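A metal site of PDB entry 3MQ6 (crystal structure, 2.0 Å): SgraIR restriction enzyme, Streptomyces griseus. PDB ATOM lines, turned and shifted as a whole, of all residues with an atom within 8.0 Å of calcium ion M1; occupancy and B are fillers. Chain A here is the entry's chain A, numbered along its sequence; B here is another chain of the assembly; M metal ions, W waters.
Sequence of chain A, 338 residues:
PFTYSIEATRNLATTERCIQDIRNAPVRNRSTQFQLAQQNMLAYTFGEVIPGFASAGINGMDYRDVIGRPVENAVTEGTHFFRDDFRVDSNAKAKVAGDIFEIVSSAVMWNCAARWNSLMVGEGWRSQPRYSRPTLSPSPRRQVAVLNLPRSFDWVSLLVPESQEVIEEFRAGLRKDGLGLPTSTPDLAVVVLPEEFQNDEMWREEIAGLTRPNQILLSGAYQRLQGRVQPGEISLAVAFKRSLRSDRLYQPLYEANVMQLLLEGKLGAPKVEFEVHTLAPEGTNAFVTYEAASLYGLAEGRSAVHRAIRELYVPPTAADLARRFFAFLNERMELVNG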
ATOM      1  N   ASP A  99       9.589  -2.289  11.039  1.00  0.00           N
ATOM      2  CA  ASP A  99       9.313  -2.973  12.295  1.00  0.00           C
ATOM      3  C   ASP A  99      10.622  -3.469  12.922  1.00  0.00           C
ATOM      4  O   ASP A  99      10.844  -3.381  14.130  1.00  0.00           O
ATOM      5  CB  ASP A  99       8.345  -4.148  12.075  1.00  0.00           C
ATOM      6  CG  ASP A  99       6.892  -3.707  11.935  1.00  0.00           C
ATOM      7  OD1 ASP A  99       6.618  -2.485  11.773  1.00  0.00           O
ATOM      8  OD2 ASP A  99       6.000  -4.590  11.978  1.00  0.00           O
ATOM      9  N   GLU A 102      12.549  -0.771  14.577  1.00  0.00           N
ATOM     10  CA  GLU A 102      11.931  -0.411  15.835  1.00  0.00           C
ATOM     11  C   GLU A 102      12.167  -1.480  16.880  1.00  0.00           C
ATOM     12  O   GLU A 102      12.542  -1.178  18.006  1.00  0.00           O
ATOM     13  CB  GLU A 102      10.442  -0.254  15.649  1.00  0.00           C
ATOM     14  CG  GLU A 102       9.765   0.148  16.907  1.00  0.00           C
ATOM     15  CD  GLU A 102       8.355  -0.373  16.997  1.00  0.00           C
ATOM     16  OE1 GLU A 102       7.937  -1.185  16.134  1.00  0.00           O
ATOM     17  OE2 GLU A 102       7.653   0.045  17.960  1.00  0.00           O
ATOM     18  N   ILE A 103      11.934  -2.742  16.516  1.00  0.00           N
ATOM     19  CA  ILE A 103      12.047  -3.836  17.497  1.00  0.00           C
ATOM     20  C   ILE A 103      13.477  -3.987  17.993  1.00  0.00           C
ATOM     21  O   ILE A 103      13.725  -4.175  19.187  1.00  0.00           O
ATOM     22  CB  ILE A 103      11.559  -5.157  16.923  1.00  0.00           C
ATOM     23  CG1 ILE A 103      10.064  -5.056  16.628  1.00  0.00           C
ATOM     24  CG2 ILE A 103      11.849  -6.317  17.875  1.00  0.00           C
ATOM     25  CD1 ILE A 103       9.512  -6.168  15.793  1.00  0.00           C
ATOM     26  N   SER A 106      14.645  -1.071  20.227  1.00  0.00           N
ATOM     27  CA  SER A 106      13.959  -1.171  21.520  1.00  0.00           C
ATOM     28  C   SER A 106      14.579  -2.261  22.378  1.00  0.00           C
ATOM     29  O   SER A 106      14.472  -2.225  23.606  1.00  0.00           O
ATOM     30  CB  SER A 106      12.477  -1.422  21.333  1.00  0.00           C
ATOM     31  OG  SER A 106      11.916  -0.334  20.620  1.00  0.00           O
ATOM     32  N   LEU A 147       9.381   0.262  27.365  1.00  0.00           N
ATOM     33  CA  LEU A 147       8.127  -0.283  26.880  1.00  0.00           C
ATOM     34  C   LEU A 147       7.929  -0.038  25.384  1.00  0.00           C
ATOM     35  O   LEU A 147       7.560   1.069  24.969  1.00  0.00           O
ATOM     36  CB  LEU A 147       6.956   0.323  27.638  1.00  0.00           C
ATOM     37  CG  LEU A 147       7.007   0.304  29.156  1.00  0.00           C
ATOM     38  CD1 LEU A 147       5.657   0.803  29.680  1.00  0.00           C
ATOM     39  CD2 LEU A 147       7.316  -1.138  29.633  1.00  0.00           C
ATOM     40  N   ASN A 148       8.153  -1.083  24.610  1.00  0.00           N
ATOM     41  CA  ASN A 148       7.811  -1.082  23.196  1.00  0.00           C
ATOM     42  C   ASN A 148       6.305  -1.199  23.089  1.00  0.00           C
ATOM     43  O   ASN A 148       5.740  -2.225  23.440  1.00  0.00           O
ATOM     44  CB  ASN A 148       8.504  -2.252  22.492  1.00  0.00           C
ATOM     45  CG  ASN A 148       8.045  -2.412  21.070  1.00  0.00           C
ATOM     46  OD1 ASN A 148       7.201  -1.659  20.624  1.00  0.00           O
ATOM     47  ND2 ASN A 148       8.609  -3.365  20.342  1.00  0.00           N
ATOM     48  N   LEU A 149       5.663  -0.140  22.596  1.00  0.00           N
ATOM     49  CA  LEU A 149       4.207  -0.050  22.631  1.00  0.00           C
ATOM     50  C   LEU A 149       3.616  -0.639  21.360  1.00  0.00           C
ATOM     51  O   LEU A 149       4.111  -0.394  20.270  1.00  0.00           O
ATOM     52  CB  LEU A 149       3.780   1.416  22.806  1.00  0.00           C
ATOM     53  CG  LEU A 149       4.379   2.137  24.021  1.00  0.00           C
ATOM     54  CD1 LEU A 149       4.030   3.628  24.047  1.00  0.00           C
ATOM     55  CD2 LEU A 149       3.876   1.479  25.286  1.00  0.00           C
ATOM     56  N   PRO A 150       2.534  -1.403  21.492  1.00  0.00           N
ATOM     57  CA  PRO A 150       1.975  -2.193  20.388  1.00  0.00           C
ATOM     58  C   PRO A 150       1.173  -1.336  19.442  1.00  0.00           C
ATOM     59  O   PRO A 150       0.812  -0.215  19.775  1.00  0.00           O
ATOM     60  CB  PRO A 150       0.994  -3.097  21.118  1.00  0.00           C
ATOM     61  CG  PRO A 150       0.455  -2.186  22.176  1.00  0.00           C
ATOM     62  CD  PRO A 150       1.657  -1.450  22.677  1.00  0.00           C
ATOM     63  N   ARG A 151       0.875  -1.900  18.269  1.00  0.00           N
ATOM     64  CA  ARG A 151       0.008  -1.243  17.328  1.00  0.00           C
ATOM     65  C   ARG A 151      -1.341  -1.064  17.985  1.00  0.00           C
ATOM     66  O   ARG A 151      -1.807  -1.949  18.716  1.00  0.00           O
ATOM     67  CB  ARG A 151      -0.136  -2.075  16.037  1.00  0.00           C
ATOM     68  CG  ARG A 151       1.076  -1.984  15.113  1.00  0.00           C
ATOM     69  CD  ARG A 151       0.855  -2.708  13.780  1.00  0.00           C
ATOM     70  NE  ARG A 151       1.725  -2.150  12.730  1.00  0.00           N
ATOM     71  CZ  ARG A 151       2.986  -2.507  12.522  1.00  0.00           C
ATOM     72  NH1 ARG A 151       3.548  -3.434  13.279  1.00  0.00           N
ATOM     73  NH2 ARG A 151       3.681  -1.947  11.549  1.00  0.00           N
ATOM     74  N   SER A 152      -1.941   0.098  17.741  1.00  0.00           N
ATOM     75  CA  SER A 152      -3.280   0.392  18.261  1.00  0.00           C
ATOM     76  C   SER A 152      -3.300   0.894  19.710  1.00  0.00           C
ATOM     77  O   SER A 152      -4.365   1.139  20.252  1.00  0.00           O
ATOM     78  CB  SER A 152      -4.167  -0.841  18.114  1.00  0.00           C
ATOM     79  OG  SER A 152      -5.531  -0.461  18.097  1.00  0.00           O
ATOM     80  N   PHE A 153      -2.133   1.020  20.345  1.00  0.00           N
ATOM     81  CA  PHE A 153      -2.065   1.479  21.744  1.00  0.00           C
ATOM     82  C   PHE A 153      -2.601   2.896  21.969  1.00  0.00           C
ATOM     83  O   PHE A 153      -2.613   3.729  21.062  1.00  0.00           O
ATOM     84  CB  PHE A 153      -0.617   1.415  22.249  1.00  0.00           C
ATOM     85  CG  PHE A 153      -0.488   1.377  23.764  1.00  0.00           C
ATOM     86  CD1 PHE A 153      -1.142   0.398  24.498  1.00  0.00           C
ATOM     87  CD2 PHE A 153       0.292   2.313  24.430  1.00  0.00           C
ATOM     88  CE1 PHE A 153      -1.018   0.361  25.876  1.00  0.00           C
ATOM     89  CE2 PHE A 153       0.420   2.268  25.806  1.00  0.00           C
ATOM     90  CZ  PHE A 153      -0.247   1.275  26.526  1.00  0.00           C
ATOM     91  N   THR A 185      -0.065   7.170  20.165  1.00  0.00           N
ATOM     92  CA  THR A 185       1.047   6.475  20.779  1.00  0.00           C
ATOM     93  C   THR A 185       2.407   6.708  20.109  1.00  0.00           C
ATOM     94  O   THR A 185       2.509   6.694  18.879  1.00  0.00           O
ATOM     95  CB  THR A 185       0.769   4.961  20.865  1.00  0.00           C
ATOM     96  OG1 THR A 185       1.727   4.356  21.726  1.00  0.00           O
ATOM     97  CG2 THR A 185       0.844   4.311  19.475  1.00  0.00           C
ATOM     98  N   PRO A 186       3.455   6.912  20.913  1.00  0.00           N
ATOM     99  CA  PRO A 186       4.824   6.815  20.409  1.00  0.00           C
ATOM    100  C   PRO A 186       5.121   5.347  20.192  1.00  0.00           C
ATOM    101  O   PRO A 186       4.290   4.540  20.611  1.00  0.00           O
ATOM    102  CB  PRO A 186       5.645   7.350  21.595  1.00  0.00           C
ATOM    103  CG  PRO A 186       4.792   7.009  22.778  1.00  0.00           C
ATOM    104  CD  PRO A 186       3.414   7.296  22.333  1.00  0.00           C
ATOM    105  N   ASP A 187       6.260   4.995  19.594  1.00  0.00           N
ATOM    106  CA  ASP A 187       6.651   3.597  19.407  1.00  0.00           C
ATOM    107  C   ASP A 187       7.067   3.002  20.715  1.00  0.00           C
ATOM    108  O   ASP A 187       6.859   1.808  20.979  1.00  0.00           O
ATOM    109  CB  ASP A 187       7.851   3.477  18.465  1.00  0.00           C
ATOM    110  CG  ASP A 187       7.489   3.808  17.026  1.00  0.00           C
ATOM    111  OD1 ASP A 187       6.410   3.372  16.577  1.00  0.00           O
ATOM    112  OD2 ASP A 187       8.283   4.508  16.371  1.00  0.00           O
ATOM    113  N   LEU A 188       7.660   3.856  21.540  1.00  0.00           N
ATOM    114  CA  LEU A 188       8.297   3.434  22.769  1.00  0.00           C
ATOM    115  C   LEU A 188       8.157   4.480  23.872  1.00  0.00           C
ATOM    116  O   LEU A 188       8.114   5.692  23.602  1.00  0.00           O
ATOM    117  CB  LEU A 188       9.760   3.114  22.481  1.00  0.00           C
ATOM    118  CG  LEU A 188      10.707   2.740  23.619  1.00  0.00           C
ATOM    119  CD1 LEU A 188      11.833   1.843  23.103  1.00  0.00           C
ATOM    120  CD2 LEU A 188      11.250   3.984  24.281  1.00  0.00           C
ATOM    121  N   LEU A 218       9.523  -8.608  25.481  1.00  0.00           N
ATOM    122  CA  LEU A 218       9.649  -7.169  25.178  1.00  0.00           C
ATOM    123  C   LEU A 218       8.381  -6.513  24.650  1.00  0.00           C
ATOM    124  O   LEU A 218       8.077  -5.369  24.995  1.00  0.00           O
ATOM    125  CB  LEU A 218      10.794  -6.924  24.194  1.00  0.00           C
ATOM    126  CG  LEU A 218      12.141  -6.764  24.911  1.00  0.00           C
ATOM    127  CD1 LEU A 218      12.359  -7.901  25.896  1.00  0.00           C
ATOM    128  CD2 LEU A 218      13.317  -6.668  23.925  1.00  0.00           C
ATOM    129  N   SER A 219       7.654  -7.239  23.808  1.00  0.00           N
ATOM    130  CA  SER A 219       6.490  -6.686  23.127  1.00  0.00           C
ATOM    131  C   SER A 219       5.233  -6.666  24.012  1.00  0.00           C
ATOM    132  O   SER A 219       4.279  -5.974  23.706  1.00  0.00           O
ATOM    133  CB  SER A 219       6.224  -7.401  21.806  1.00  0.00           C
ATOM    134  OG  SER A 219       5.498  -8.613  21.970  1.00  0.00           O
ATOM    135  N   PHE A 240      10.432   5.844  16.124  1.00  0.00           N
ATOM    136  CA  PHE A 240      11.404   5.346  15.164  1.00  0.00           C
ATOM    137  C   PHE A 240      10.847   5.413  13.761  1.00  0.00           C
ATOM    138  O   PHE A 240       9.762   4.949  13.502  1.00  0.00           O
ATOM    139  CB  PHE A 240      11.721   3.873  15.455  1.00  0.00           C
ATOM    140  CG  PHE A 240      12.318   3.645  16.805  1.00  0.00           C
ATOM    141  CD1 PHE A 240      13.681   3.858  17.031  1.00  0.00           C
ATOM    142  CD2 PHE A 240      11.533   3.232  17.863  1.00  0.00           C
ATOM    143  CE1 PHE A 240      14.229   3.653  18.289  1.00  0.00           C
ATOM    144  CE2 PHE A 240      12.076   3.029  19.108  1.00  0.00           C
ATOM    145  CZ  PHE A 240      13.425   3.242  19.317  1.00  0.00           C
ATOM    146  P    DA B   7      -2.046   2.482  14.951  1.00  0.00           P
ATOM    147  OP1  DA B   7      -1.558   2.500  16.350  1.00  0.00           O
ATOM    148  OP2  DA B   7      -2.830   3.577  14.396  1.00  0.00           O
ATOM    149  O5'  DA B   7      -0.773   2.287  14.020  1.00  0.00           O
ATOM    150  C5'  DA B   7       0.279   1.460  14.471  1.00  0.00           C
ATOM    151  C4'  DA B   7       1.307   1.369  13.379  1.00  0.00           C
ATOM    152  O4'  DA B   7       0.679   0.824  12.192  1.00  0.00           O
ATOM    153  C3'  DA B   7       1.882   2.724  12.953  1.00  0.00           C
ATOM    154  O3'  DA B   7       3.259   2.537  12.978  1.00  0.00           O
ATOM    155  C2'  DA B   7       1.346   2.960  11.535  1.00  0.00           C
ATOM    156  C1'  DA B   7       1.137   1.524  11.069  1.00  0.00           C
ATOM    157  N9   DA B   7       0.139   1.281  10.029  1.00  0.00           N
ATOM    158  C8   DA B   7      -1.038   1.928   9.802  1.00  0.00           C
ATOM    159  N7   DA B   7      -1.709   1.437   8.789  1.00  0.00           N
ATOM    160  C5   DA B   7      -0.930   0.407   8.324  1.00  0.00           C
ATOM    161  C6   DA B   7      -1.081  -0.477   7.258  1.00  0.00           C
ATOM    162  N6   DA B   7      -2.134  -0.480   6.446  1.00  0.00           N
ATOM    163  N1   DA B   7      -0.109  -1.381   7.056  1.00  0.00           N
ATOM    164  C2   DA B   7       0.948  -1.387   7.864  1.00  0.00           C
ATOM    165  N3   DA B   7       1.214  -0.584   8.893  1.00  0.00           N
ATOM    166  C4   DA B   7       0.228   0.300   9.066  1.00  0.00           C
ATOM    167  P    DC B   8       4.370   3.573  12.476  1.00  0.00           P
ATOM    168  OP1  DC B   8       5.279   3.692  13.628  1.00  0.00           O
ATOM    169  OP2  DC B   8       3.750   4.793  11.926  1.00  0.00           O
ATOM    170  O5'  DC B   8       5.105   2.675  11.358  1.00  0.00           O
ATOM    171  C5'  DC B   8       5.887   1.535  11.751  1.00  0.00           C
ATOM    172  C4'  DC B   8       6.289   0.752  10.515  1.00  0.00           C
ATOM    173  O4'  DC B   8       5.105   0.231   9.876  1.00  0.00           O
ATOM    174  C3'  DC B   8       6.919   1.639   9.435  1.00  0.00           C
ATOM    175  O3'  DC B   8       8.297   1.800   9.724  1.00  0.00           O
ATOM    176  C2'  DC B   8       6.674   0.823   8.187  1.00  0.00           C
ATOM    177  C1'  DC B   8       5.285   0.236   8.480  1.00  0.00           C
ATOM    178  N1   DC B   8       4.134   0.937   7.891  1.00  0.00           N
ATOM    179  C2   DC B   8       3.739   0.497   6.639  1.00  0.00           C
ATOM    180  O2   DC B   8       4.374  -0.432   6.126  1.00  0.00           O
ATOM    181  N3   DC B   8       2.681   1.095   6.040  1.00  0.00           N
ATOM    182  C4   DC B   8       2.034   2.075   6.652  1.00  0.00           C
ATOM    183  N4   DC B   8       0.980   2.601   6.000  1.00  0.00           N
ATOM    184  C5   DC B   8       2.431   2.547   7.947  1.00  0.00           C
ATOM    185  C6   DC B   8       3.483   1.951   8.533  1.00  0.00           C
HETATM  186 CA    CA M   1       5.789  -1.387  18.709  1.00  0.00          CA
HETATM  187 CA    CA M   2       7.437   4.304  14.092  1.00  0.00          CA
HETATM  188  O   HOH W   1       6.919  -3.632  17.559  1.00  0.00           O
HETATM  189  O   HOH W   2       4.927  -4.142  19.037  1.00  0.00           O
HETATM  190  O   HOH W   3       4.913   1.049  17.327  1.00  0.00           O
HETATM  191  O   HOH W   4       4.653  -2.282  16.694  1.00  0.00           O
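O of Glu 102 lies within hydrogen-bond range of OG of Ser 106 (2.8 Å). N of Leu 149 sits at hydrogen-bond distance from O of Asp 187.
Within 4 Å of calcium ion M1: Glu 102, Asn 148 and Leu 149. The nearest printed residue that does not touch calcium ion M1 is Asp 187 (4.1 Å).
Calcium ion M1 is bound by OD1 of Asn 148, 2.4 Å away. Calcium ion M1 is bound by OE2 of Glu 102. Calcium ion M1 is bound by water W4 (2.5 Å). The backbone carbonyl oxygen (O) of Leu 149 binds calcium ion M1, 2.5 Å away. Calcium ion M1 is bound by water W1 (2.8 Å). Calcium ion M1 has five donor atoms within binding distance. Slightly farther from calcium ion M1 lies water W2 (2.9 Å). Slightly farther from calcium ion M1 lies water W3 (2.9 Å).
Water W1 lies within hydrogen-bond range of OE1 of Glu 102 (3.0 Å) and ND2 of Asn 148 (3.3 Å).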
